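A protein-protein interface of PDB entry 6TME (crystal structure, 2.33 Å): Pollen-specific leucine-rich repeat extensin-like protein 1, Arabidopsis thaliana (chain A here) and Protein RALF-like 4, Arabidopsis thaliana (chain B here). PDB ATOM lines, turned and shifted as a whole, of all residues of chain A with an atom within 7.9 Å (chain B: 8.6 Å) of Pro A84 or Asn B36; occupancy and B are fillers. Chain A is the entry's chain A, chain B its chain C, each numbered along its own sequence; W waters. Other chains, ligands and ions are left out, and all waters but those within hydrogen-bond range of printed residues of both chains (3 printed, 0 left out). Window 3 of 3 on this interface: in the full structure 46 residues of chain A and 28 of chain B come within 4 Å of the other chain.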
ATOM      1  N   ARG A  43      16.670  -1.364  36.951  1.00  0.00           N
ATOM      2  CA  ARG A  43      16.424  -1.104  35.538  1.00  0.00           C
ATOM      3  C   ARG A  43      17.606  -0.404  34.868  1.00  0.00           C
ATOM      4  O   ARG A  43      18.006  -0.775  33.753  1.00  0.00           O
ATOM      5  CB  ARG A  43      15.144  -0.284  35.419  1.00  0.00           C
ATOM      6  CG  ARG A  43      14.826   0.284  34.087  1.00  0.00           C
ATOM      7  CD  ARG A  43      13.455   0.945  34.131  1.00  0.00           C
ATOM      8  NE  ARG A  43      12.436   0.054  34.665  1.00  0.00           N
ATOM      9  CZ  ARG A  43      11.202  -0.052  34.182  1.00  0.00           C
ATOM     10  NH1 ARG A  43      10.831   0.674  33.134  1.00  0.00           N
ATOM     11  NH2 ARG A  43      10.338  -0.888  34.748  1.00  0.00           N
ATOM     12  N   PHE A  81      20.177   8.670  25.689  1.00  0.00           N
ATOM     13  CA  PHE A  81      19.184   9.699  25.978  1.00  0.00           C
ATOM     14  C   PHE A  81      18.094   9.124  26.864  1.00  0.00           C
ATOM     15  O   PHE A  81      17.406   8.181  26.483  1.00  0.00           O
ATOM     16  CB  PHE A  81      18.622  10.278  24.683  1.00  0.00           C
ATOM     17  CG  PHE A  81      19.661  11.034  23.874  1.00  0.00           C
ATOM     18  CD1 PHE A  81      19.850  12.400  24.064  1.00  0.00           C
ATOM     19  CD2 PHE A  81      20.484  10.366  22.971  1.00  0.00           C
ATOM     20  CE1 PHE A  81      20.808  13.099  23.342  1.00  0.00           C
ATOM     21  CE2 PHE A  81      21.452  11.053  22.251  1.00  0.00           C
ATOM     22  CZ  PHE A  81      21.602  12.439  22.432  1.00  0.00           C
ATOM     23  N   CYS A  82      17.945   9.694  28.048  1.00  0.00           N
ATOM     24  CA  CYS A  82      17.021   9.205  29.056  1.00  0.00           C
ATOM     25  C   CYS A  82      15.743  10.036  29.019  1.00  0.00           C
ATOM     26  O   CYS A  82      15.675  11.087  28.378  1.00  0.00           O
ATOM     27  CB  CYS A  82      17.665   9.232  30.450  1.00  0.00           C
ATOM     28  SG  CYS A  82      18.907   7.917  30.722  1.00  0.00           S
ATOM     29  N   ALA A  83      14.721   9.536  29.705  1.00  0.00           N
ATOM     30  CA  ALA A  83      13.373  10.087  29.640  1.00  0.00           C
ATOM     31  C   ALA A  83      12.540   9.456  30.755  1.00  0.00           C
ATOM     32  O   ALA A  83      12.926   8.421  31.307  1.00  0.00           O
ATOM     33  CB  ALA A  83      12.719   9.818  28.272  1.00  0.00           C
ATOM     34  N   PRO A  84      11.402  10.059  31.089  1.00  0.00           N
ATOM     35  CA  PRO A  84      10.468   9.399  32.003  1.00  0.00           C
ATOM     36  C   PRO A  84       9.862   8.176  31.344  1.00  0.00           C
ATOM     37  O   PRO A  84       9.625   8.154  30.134  1.00  0.00           O
ATOM     38  CB  PRO A  84       9.395  10.471  32.268  1.00  0.00           C
ATOM     39  CG  PRO A  84       9.978  11.763  31.780  1.00  0.00           C
ATOM     40  CD  PRO A  84      10.921  11.389  30.667  1.00  0.00           C
ATOM     41  N   ALA A  85       9.603   7.153  32.155  1.00  0.00           N
ATOM     42  CA  ALA A  85       8.909   5.978  31.644  1.00  0.00           C
ATOM     43  C   ALA A  85       7.556   6.369  31.066  1.00  0.00           C
ATOM     44  O   ALA A  85       6.886   7.289  31.556  1.00  0.00           O
ATOM     45  CB  ALA A  85       8.722   4.936  32.743  1.00  0.00           C
ATOM     46  N   LEU A  86       7.155   5.659  30.005  1.00  0.00           N
ATOM     47  CA  LEU A  86       5.881   5.963  29.355  1.00  0.00           C
ATOM     48  C   LEU A  86       4.709   5.744  30.295  1.00  0.00           C
ATOM     49  O   LEU A  86       3.733   6.502  30.263  1.00  0.00           O
ATOM     50  CB  LEU A  86       5.710   5.111  28.105  1.00  0.00           C
ATOM     51  CG  LEU A  86       6.564   5.607  26.943  1.00  0.00           C
ATOM     52  CD1 LEU A  86       6.343   4.728  25.715  1.00  0.00           C
ATOM     53  CD2 LEU A  86       6.212   7.046  26.673  1.00  0.00           C
ATOM     54  N   ASP A  87       4.788   4.712  31.138  1.00  0.00           N
ATOM     55  CA  ASP A  87       3.723   4.339  32.052  1.00  0.00           C
ATOM     56  C   ASP A  87       3.925   4.879  33.469  1.00  0.00           C
ATOM     57  O   ASP A  87       3.152   4.524  34.358  1.00  0.00           O
ATOM     58  CB  ASP A  87       3.607   2.818  32.107  1.00  0.00           C
ATOM     59  CG  ASP A  87       4.957   2.147  32.230  1.00  0.00           C
ATOM     60  OD1 ASP A  87       5.955   2.756  31.779  1.00  0.00           O
ATOM     61  OD2 ASP A  87       5.030   1.022  32.775  1.00  0.00           O
ATOM     62  N   ASP A  88       4.945   5.714  33.704  1.00  0.00           N
ATOM     63  CA  ASP A  88       5.241   6.242  35.037  1.00  0.00           C
ATOM     64  C   ASP A  88       6.282   7.348  34.931  1.00  0.00           C
ATOM     65  O   ASP A  88       7.484   7.064  34.869  1.00  0.00           O
ATOM     66  CB  ASP A  88       5.741   5.131  35.975  1.00  0.00           C
ATOM     67  CG  ASP A  88       5.764   5.557  37.461  1.00  0.00           C
ATOM     68  OD1 ASP A  88       5.517   6.752  37.764  1.00  0.00           O
ATOM     69  OD2 ASP A  88       6.031   4.682  38.329  1.00  0.00           O
ATOM     70  N   PRO A  89       5.872   8.619  34.921  1.00  0.00           N
ATOM     71  CA  PRO A  89       6.839   9.712  34.732  1.00  0.00           C
ATOM     72  C   PRO A  89       7.793   9.933  35.907  1.00  0.00           C
ATOM     73  O   PRO A  89       8.650  10.821  35.826  1.00  0.00           O
ATOM     74  CB  PRO A  89       5.935  10.935  34.522  1.00  0.00           C
ATOM     75  CG  PRO A  89       4.679  10.590  35.237  1.00  0.00           C
ATOM     76  CD  PRO A  89       4.492   9.111  35.064  1.00  0.00           C
ATOM     77  N   SER A  90       7.686   9.175  36.993  1.00  0.00           N
ATOM     78  CA  SER A  90       8.644   9.265  38.085  1.00  0.00           C
ATOM     79  C   SER A  90       9.804   8.277  37.948  1.00  0.00           C
ATOM     80  O   SER A  90      10.769   8.355  38.718  1.00  0.00           O
ATOM     81  CB  SER A  90       7.930   9.030  39.412  1.00  0.00           C
ATOM     82  OG  SER A  90       7.660   7.654  39.561  1.00  0.00           O
ATOM     83  N   VAL A  91       9.734   7.352  36.999  1.00  0.00           N
ATOM     84  CA  VAL A  91      10.818   6.418  36.717  1.00  0.00           C
ATOM     85  C   VAL A  91      11.642   6.919  35.532  1.00  0.00           C
ATOM     86  O   VAL A  91      11.093   7.419  34.538  1.00  0.00           O
ATOM     87  CB  VAL A  91      10.263   5.007  36.463  1.00  0.00           C
ATOM     88  CG1 VAL A  91      11.398   4.062  36.032  1.00  0.00           C
ATOM     89  CG2 VAL A  91       9.559   4.509  37.731  1.00  0.00           C
ATOM     90  N   LEU A  92      12.964   6.802  35.656  1.00  0.00           N
ATOM     91  CA  LEU A  92      13.935   7.201  34.645  1.00  0.00           C
ATOM     92  C   LEU A  92      14.335   5.982  33.828  1.00  0.00           C
ATOM     93  O   LEU A  92      14.679   4.949  34.409  1.00  0.00           O
ATOM     94  CB  LEU A  92      15.183   7.798  35.301  1.00  0.00           C
ATOM     95  CG  LEU A  92      16.245   8.437  34.391  1.00  0.00           C
ATOM     96  CD1 LEU A  92      15.689   9.678  33.701  1.00  0.00           C
ATOM     97  CD2 LEU A  92      17.503   8.782  35.192  1.00  0.00           C
ATOM     98  N   VAL A  93      14.298   6.106  32.488  1.00  0.00           N
ATOM     99  CA  VAL A  93      14.641   5.009  31.578  1.00  0.00           C
ATOM    100  C   VAL A  93      15.521   5.524  30.446  1.00  0.00           C
ATOM    101  O   VAL A  93      15.503   6.713  30.109  1.00  0.00           O
ATOM    102  CB  VAL A  93      13.390   4.310  30.977  1.00  0.00           C
ATOM    103  CG1 VAL A  93      12.430   3.829  32.068  1.00  0.00           C
ATOM    104  CG2 VAL A  93      12.673   5.220  29.970  1.00  0.00           C
ATOM    105  N   VAL A  94      16.313   4.617  29.874  1.00  0.00           N
ATOM    106  CA  VAL A  94      17.055   4.887  28.643  1.00  0.00           C
ATOM    107  C   VAL A  94      16.091   4.669  27.479  1.00  0.00           C
ATOM    108  O   VAL A  94      15.678   3.539  27.200  1.00  0.00           O
ATOM    109  CB  VAL A  94      18.299   3.996  28.513  1.00  0.00           C
ATOM    110  CG1 VAL A  94      18.922   4.144  27.123  1.00  0.00           C
ATOM    111  CG2 VAL A  94      19.331   4.335  29.591  1.00  0.00           C
ATOM    112  N   ALA A  95      15.731   5.751  26.801  1.00  0.00           N
ATOM    113  CA  ALA A  95      14.685   5.735  25.791  1.00  0.00           C
ATOM    114  C   ALA A  95      15.233   5.895  24.394  1.00  0.00           C
ATOM    115  O   ALA A  95      14.510   5.627  23.420  1.00  0.00           O
ATOM    116  CB  ALA A  95      13.661   6.861  26.050  1.00  0.00           C
ATOM    117  N   GLY A  96      16.480   6.323  24.274  1.00  0.00           N
ATOM    118  CA  GLY A  96      17.031   6.637  22.981  1.00  0.00           C
ATOM    119  C   GLY A  96      18.528   6.439  22.922  1.00  0.00           C
ATOM    120  O   GLY A  96      19.247   6.645  23.904  1.00  0.00           O
ATOM    121  N   ASP A 117      13.602  -0.236  27.143  1.00  0.00           N
ATOM    122  CA  ASP A 117      12.806   0.979  27.026  1.00  0.00           C
ATOM    123  C   ASP A 117      13.144   1.797  25.786  1.00  0.00           C
ATOM    124  O   ASP A 117      12.534   2.846  25.571  1.00  0.00           O
ATOM    125  CB  ASP A 117      12.983   1.840  28.289  1.00  0.00           C
ATOM    126  CG  ASP A 117      12.581   1.088  29.559  1.00  0.00           C
ATOM    127  OD1 ASP A 117      11.452   0.546  29.576  1.00  0.00           O
ATOM    128  OD2 ASP A 117      13.408   0.990  30.507  1.00  0.00           O
ATOM    129  N   LEU A 120      14.044   4.838  20.236  1.00  0.00           N
ATOM    130  CA  LEU A 120      14.755   5.563  19.201  1.00  0.00           C
ATOM    131  C   LEU A 120      16.159   4.995  19.125  1.00  0.00           C
ATOM    132  O   LEU A 120      16.868   4.938  20.139  1.00  0.00           O
ATOM    133  CB  LEU A 120      14.764   7.052  19.515  1.00  0.00           C
ATOM    134  CG  LEU A 120      15.432   8.040  18.575  1.00  0.00           C
ATOM    135  CD1 LEU A 120      14.663   9.321  18.772  1.00  0.00           C
ATOM    136  CD2 LEU A 120      16.935   8.236  18.910  1.00  0.00           C
ATOM    137  N   GLU A 144      11.581   3.948  15.733  1.00  0.00           N
ATOM    138  CA  GLU A 144      12.429   4.435  14.647  1.00  0.00           C
ATOM    139  C   GLU A 144      13.802   3.795  14.778  1.00  0.00           C
ATOM    140  O   GLU A 144      14.525   4.037  15.751  1.00  0.00           O
ATOM    141  CB  GLU A 144      12.570   5.966  14.625  1.00  0.00           C
ATOM    142  CG  GLU A 144      12.774   6.652  15.956  1.00  0.00           C
ATOM    143  CD  GLU A 144      12.686   8.179  15.856  1.00  0.00           C
ATOM    144  OE1 GLU A 144      13.584   8.823  15.262  1.00  0.00           O
ATOM    145  OE2 GLU A 144      11.686   8.729  16.367  1.00  0.00           O
ATOM    146  N   ARG B  22      20.882  15.628  17.923  1.00  0.00           N
ATOM    147  CA  ARG B  22      21.168  14.304  18.452  1.00  0.00           C
ATOM    148  C   ARG B  22      20.190  13.935  19.565  1.00  0.00           C
ATOM    149  O   ARG B  22      20.043  14.668  20.548  1.00  0.00           O
ATOM    150  CB  ARG B  22      22.607  14.284  18.960  1.00  0.00           C
ATOM    151  CG  ARG B  22      23.290  12.937  18.957  1.00  0.00           C
ATOM    152  CD  ARG B  22      24.681  13.066  19.568  1.00  0.00           C
ATOM    153  NE  ARG B  22      24.644  13.098  21.033  1.00  0.00           N
ATOM    154  CZ  ARG B  22      25.168  14.065  21.786  1.00  0.00           C
ATOM    155  NH1 ARG B  22      25.075  13.994  23.113  1.00  0.00           N
ATOM    156  NH2 ARG B  22      25.788  15.095  21.214  1.00  0.00           N
ATOM    157  N   GLY B  23      19.521  12.796  19.414  1.00  0.00           N
ATOM    158  CA  GLY B  23      18.609  12.306  20.422  1.00  0.00           C
ATOM    159  C   GLY B  23      17.145  12.592  20.151  1.00  0.00           C
ATOM    160  O   GLY B  23      16.282  11.994  20.810  1.00  0.00           O
ATOM    161  N   ARG B  24      16.841  13.463  19.192  1.00  0.00           N
ATOM    162  CA  ARG B  24      15.468  13.808  18.862  1.00  0.00           C
ATOM    163  C   ARG B  24      14.879  12.841  17.849  1.00  0.00           C
ATOM    164  O   ARG B  24      15.576  12.330  16.966  1.00  0.00           O
ATOM    165  CB  ARG B  24      15.390  15.229  18.302  1.00  0.00           C
ATOM    166  CG  ARG B  24      15.605  16.256  19.382  1.00  0.00           C
ATOM    167  CD  ARG B  24      15.113  17.616  18.993  1.00  0.00           C
ATOM    168  NE  ARG B  24      15.588  18.557  19.987  1.00  0.00           N
ATOM    169  CZ  ARG B  24      15.011  18.726  21.167  1.00  0.00           C
ATOM    170  NH1 ARG B  24      13.919  18.033  21.473  1.00  0.00           N
ATOM    171  NH2 ARG B  24      15.519  19.594  22.035  1.00  0.00           N
ATOM    172  N   SER B  25      13.575  12.616  17.965  1.00  0.00           N
ATOM    173  CA  SER B  25      12.877  11.833  16.955  1.00  0.00           C
ATOM    174  C   SER B  25      12.961  12.525  15.601  1.00  0.00           C
ATOM    175  O   SER B  25      12.893  13.761  15.505  1.00  0.00           O
ATOM    176  CB  SER B  25      11.420  11.628  17.335  1.00  0.00           C
ATOM    177  OG  SER B  25      10.740  10.910  16.330  1.00  0.00           O
ATOM    178  N   TYR B  26      13.125  11.714  14.546  1.00  0.00           N
ATOM    179  CA  TYR B  26      12.977  12.217  13.186  1.00  0.00           C
ATOM    180  C   TYR B  26      11.589  12.822  12.957  1.00  0.00           C
ATOM    181  O   TYR B  26      11.394  13.588  12.010  1.00  0.00           O
ATOM    182  CB  TYR B  26      13.257  11.077  12.211  1.00  0.00           C
ATOM    183  CG  TYR B  26      14.695  10.609  12.223  1.00  0.00           C
ATOM    184  CD1 TYR B  26      15.708  11.417  12.741  1.00  0.00           C
ATOM    185  CD2 TYR B  26      15.040   9.370  11.726  1.00  0.00           C
ATOM    186  CE1 TYR B  26      17.022  11.001  12.750  1.00  0.00           C
ATOM    187  CE2 TYR B  26      16.359   8.936  11.736  1.00  0.00           C
ATOM    188  CZ  TYR B  26      17.338   9.750  12.242  1.00  0.00           C
ATOM    189  OH  TYR B  26      18.637   9.309  12.236  1.00  0.00           O
ATOM    190  N   ASP B  28      10.131  14.806  15.207  1.00  0.00           N
ATOM    191  CA  ASP B  28      10.007  15.963  16.089  1.00  0.00           C
ATOM    192  C   ASP B  28      11.327  16.729  16.106  1.00  0.00           C
ATOM    193  O   ASP B  28      11.909  16.969  17.164  1.00  0.00           O
ATOM    194  CB  ASP B  28       9.594  15.523  17.499  1.00  0.00           C
ATOM    195  CG  ASP B  28       9.330  16.706  18.439  1.00  0.00           C
ATOM    196  OD1 ASP B  28       8.471  17.540  18.102  1.00  0.00           O
ATOM    197  OD2 ASP B  28       9.968  16.803  19.518  1.00  0.00           O
ATOM    198  N   LYS B  30      12.558  19.717  16.318  1.00  0.00           N
ATOM    199  CA  LYS B  30      12.181  21.074  16.679  1.00  0.00           C
ATOM    200  C   LYS B  30      12.783  21.351  18.042  1.00  0.00           C
ATOM    201  O   LYS B  30      12.687  20.508  18.939  1.00  0.00           O
ATOM    202  CB  LYS B  30      10.659  21.241  16.705  1.00  0.00           C
ATOM    203  N   ARG B  32      13.075  22.174  21.576  1.00  0.00           N
ATOM    204  CA  ARG B  32      12.172  22.213  22.714  1.00  0.00           C
ATOM    205  C   ARG B  32      12.988  22.292  23.995  1.00  0.00           C
ATOM    206  O   ARG B  32      14.172  21.947  24.021  1.00  0.00           O
ATOM    207  CB  ARG B  32      11.246  20.987  22.752  1.00  0.00           C
ATOM    208  CG  ARG B  32      10.209  20.975  21.653  1.00  0.00           C
ATOM    209  CD  ARG B  32       9.579  19.613  21.499  1.00  0.00           C
ATOM    210  NE  ARG B  32       8.703  19.532  20.330  1.00  0.00           N
ATOM    211  CZ  ARG B  32       7.601  20.254  20.139  1.00  0.00           C
ATOM    212  NH1 ARG B  32       7.188  21.132  21.048  1.00  0.00           N
ATOM    213  NH2 ARG B  32       6.894  20.085  19.031  1.00  0.00           N
ATOM    214  N   ARG B  33      12.340  22.761  25.065  1.00  0.00           N
ATOM    215  CA  ARG B  33      13.034  22.888  26.343  1.00  0.00           C
ATOM    216  C   ARG B  33      13.610  21.553  26.800  1.00  0.00           C
ATOM    217  O   ARG B  33      14.659  21.519  27.454  1.00  0.00           O
ATOM    218  CB  ARG B  33      12.089  23.457  27.404  1.00  0.00           C
ATOM    219  N   ARG B  34      12.959  20.449  26.447  1.00  0.00           N
ATOM    220  CA  ARG B  34      13.397  19.117  26.828  1.00  0.00           C
ATOM    221  C   ARG B  34      13.675  18.286  25.581  1.00  0.00           C
ATOM    222  O   ARG B  34      13.302  18.651  24.461  1.00  0.00           O
ATOM    223  CB  ARG B  34      12.353  18.438  27.721  1.00  0.00           C
ATOM    224  CG  ARG B  34      12.147  19.155  29.044  1.00  0.00           C
ATOM    225  CD  ARG B  34      10.999  18.566  29.842  1.00  0.00           C
ATOM    226  NE  ARG B  34       9.719  18.652  29.143  1.00  0.00           N
ATOM    227  CZ  ARG B  34       8.976  19.754  29.053  1.00  0.00           C
ATOM    228  NH1 ARG B  34       9.383  20.889  29.614  1.00  0.00           N
ATOM    229  NH2 ARG B  34       7.824  19.721  28.394  1.00  0.00           N
ATOM    230  N   ASN B  35      14.349  17.150  25.791  1.00  0.00           N
ATOM    231  CA  ASN B  35      14.825  16.287  24.710  1.00  0.00           C
ATOM    232  C   ASN B  35      14.359  14.849  24.985  1.00  0.00           C
ATOM    233  O   ASN B  35      15.149  13.989  25.385  1.00  0.00           O
ATOM    234  CB  ASN B  35      16.350  16.387  24.575  1.00  0.00           C
ATOM    235  CG  ASN B  35      16.876  15.705  23.334  1.00  0.00           C
ATOM    236  OD1 ASN B  35      16.264  14.771  22.820  1.00  0.00           O
ATOM    237  ND2 ASN B  35      18.010  16.181  22.832  1.00  0.00           N
ATOM    238  N   ASN B  36      13.063  14.597  24.755  1.00  0.00           N
ATOM    239  CA  ASN B  36      12.462  13.294  25.018  1.00  0.00           C
ATOM    240  C   ASN B  36      12.372  12.475  23.729  1.00  0.00           C
ATOM    241  O   ASN B  36      11.614  12.850  22.815  1.00  0.00           O
ATOM    242  CB  ASN B  36      11.076  13.477  25.632  1.00  0.00           C
ATOM    243  CG  ASN B  36      10.487  12.172  26.163  1.00  0.00           C
ATOM    244  OD1 ASN B  36      10.905  11.076  25.776  1.00  0.00           O
ATOM    245  ND2 ASN B  36       9.529  12.288  27.080  1.00  0.00           N
ATOM    246  N   PRO B  37      13.087  11.349  23.608  1.00  0.00           N
ATOM    247  CA  PRO B  37      12.976  10.549  22.369  1.00  0.00           C
ATOM    248  C   PRO B  37      11.575  10.011  22.122  1.00  0.00           C
ATOM    249  O   PRO B  37      11.209   9.782  20.958  1.00  0.00           O
ATOM    250  CB  PRO B  37      13.999   9.418  22.580  1.00  0.00           C
ATOM    251  CG  PRO B  37      14.981   9.982  23.593  1.00  0.00           C
ATOM    252  CD  PRO B  37      14.113  10.815  24.520  1.00  0.00           C
ATOM    253  N   TYR B  38      10.765   9.838  23.172  1.00  0.00           N
ATOM    254  CA  TYR B  38       9.387   9.369  22.994  1.00  0.00           C
ATOM    255  C   TYR B  38       8.489  10.400  22.323  1.00  0.00           C
ATOM    256  O   TYR B  38       7.405  10.037  21.851  1.00  0.00           O
ATOM    257  CB  TYR B  38       8.766   8.998  24.337  1.00  0.00           C
ATOM    258  CG  TYR B  38       9.360   7.774  24.974  1.00  0.00           C
ATOM    259  CD1 TYR B  38       9.676   6.644  24.205  1.00  0.00           C
ATOM    260  CD2 TYR B  38       9.608   7.738  26.346  1.00  0.00           C
ATOM    261  CE1 TYR B  38      10.232   5.505  24.794  1.00  0.00           C
ATOM    262  CE2 TYR B  38      10.154   6.608  26.951  1.00  0.00           C
ATOM    263  CZ  TYR B  38      10.465   5.498  26.175  1.00  0.00           C
ATOM    264  OH  TYR B  38      11.007   4.393  26.773  1.00  0.00           O
ATOM    265  N   ARG B  39       8.901  11.671  22.281  1.00  0.00           N
ATOM    266  CA  ARG B  39       8.038  12.730  21.782  1.00  0.00           C
ATOM    267  C   ARG B  39       8.092  12.790  20.261  1.00  0.00           C
ATOM    268  O   ARG B  39       9.174  12.822  19.664  1.00  0.00           O
ATOM    269  CB  ARG B  39       8.422  14.087  22.368  1.00  0.00           C
ATOM    270  CG  ARG B  39       7.661  15.234  21.699  1.00  0.00           C
ATOM    271  CD  ARG B  39       7.590  16.485  22.560  1.00  0.00           C
ATOM    272  NE  ARG B  39       6.559  17.397  22.076  1.00  0.00           N
ATOM    273  CZ  ARG B  39       6.210  18.534  22.671  1.00  0.00           C
ATOM    274  NH1 ARG B  39       6.823  18.917  23.782  1.00  0.00           N
ATOM    275  NH2 ARG B  39       5.252  19.290  22.146  1.00  0.00           N
ATOM    276  N   ARG B  40       6.913  12.816  19.646  1.00  0.00           N
ATOM    277  CA  ARG B  40       6.774  12.891  18.201  1.00  0.00           C
ATOM    278  C   ARG B  40       5.838  14.043  17.848  1.00  0.00           C
ATOM    279  O   ARG B  40       5.889  15.100  18.485  1.00  0.00           O
ATOM    280  CB  ARG B  40       6.261  11.563  17.663  1.00  0.00           C
ATOM    281  CG  ARG B  40       7.339  10.531  17.421  1.00  0.00           C
ATOM    282  CD  ARG B  40       7.769   9.705  18.650  1.00  0.00           C
ATOM    283  NE  ARG B  40       6.793   8.748  19.179  1.00  0.00           N
ATOM    284  CZ  ARG B  40       7.124   7.623  19.823  1.00  0.00           C
ATOM    285  NH1 ARG B  40       8.401   7.293  19.984  1.00  0.00           N
ATOM    286  NH2 ARG B  40       6.184   6.822  20.319  1.00  0.00           N
HETATM  287  O   HOH W   1      10.495   7.891  18.674  1.00  0.00           O
HETATM  288  O   HOH W   2       8.174   9.890  28.762  1.00  0.00           O
HETATM  289  O   HOH W   3      17.323  12.862  26.952  1.00  0.00           O
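Among the printed residues, pairs that only touch across the chains: Phe A81 with Arg B22 (3.3 Å), Ala A83 with Asn B36 (3.3 Å), Ala A95 with Tyr B38 (3.5 Å), Leu A86 with Tyr B38 (3.5 Å), Leu A120 with Ser B25 (3.6 Å), Pro A84 with Tyr B38 (3.6 Å), Phe A81 with Gly B23 (3.6 Å), Leu A120 with Arg B24 (3.6 Å), Val A93 with Tyr B38 (3.7 Å), Leu A120 with Gly B23 (3.7 Å), Phe A81 with Pro B37 (3.8 Å), Leu A120 with Pro B37 (3.9 Å), Ala A95 with Pro B37 (3.9 Å), Pro A84 with Asn B36 (3.95 Å) and Gly A96 with Pro B37 (3.97 Å).
Of the 16 printed residues of chain B, 8 touch a printed residue of chain A.
Printed residues of chain A that touch a printed residue of chain B: Phe A81, Ala A83, Pro A84, Leu A86, Val A93, Ala A95, Gly A96, Asp A117, Leu A120 and Glu A144.
Among the printed residues, no Asp or Glu carboxylate lies within 4 Å of a Lys or Arg side-chain nitrogen of the other chain.
O of Asp A117 lies within hydrogen-bond range of OH of Tyr B38 (2.5 Å).
The side-chain carboxylate (OE1) of Glu A144 sits at hydrogen-bond distance from the backbone NH (N) of Tyr B26, at 3.0 Å.
The side-chain carboxylate (OE2) of Glu A144 sits close to the side-chain hydroxyl (OG) of Ser B25 (2.4 Å).
Water W1 lies within hydrogen-bond range of NH1 of Arg B40 (2.5 Å), OE2 of Glu A144 (2.7 Å) and O of Pro B37 (3.0 Å).
Water W2 lies within hydrogen-bond range of O of Pro A84 (2.6 Å) and ND2 of Asn B36 (3.2 Å).
Water W3 bridges the backbone carbonyl oxygen (O) of Cys A82 and the backbone carbonyl oxygen (O) of Asn B35.
The guanidinium group (NH1) of Arg A43 lies within salt-bridge range of the side-chain carboxylate (OD1) of Asp A117.
N of Ala A95 lies within hydrogen-bond range of O of Phe A81.
The backbone NH (N) of Phe A81 lies within hydrogen-bond range of the backbone carbonyl oxygen (O) of Gly A96.
The backbone carbonyl oxygen (O) of Ala A95 sits at hydrogen-bond distance from the backbone NH (N) of Leu A120.
The side-chain amide nitrogen of Asn B35 sits at hydrogen-bond distance from the backbone carbonyl oxygen of Arg B22 (3.4 Å).
The backbone carbonyl oxygen of Gly B23 lies close to the side-chain amide oxygen of Asn B35, at 3.4 Å.
Of chain B, only Asn B36 and Tyr B38 come within 4 Å of Pro A84.
Asn B36 touches two residues of chain A.
Printed residues of chain B within 4 Å of Ala A83: Asn B36.
Of the printed residues of chain B, Ala A95 touches Pro B37 (3.9 Å) and Tyr B38 (3.5 Å).
Of the printed residues of chain B, Leu A86 touches Tyr B38 (3.5 Å).
Asp B28 touches none of the printed residues of chain A.
Arg B33 touches none of the printed residues of chain A.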
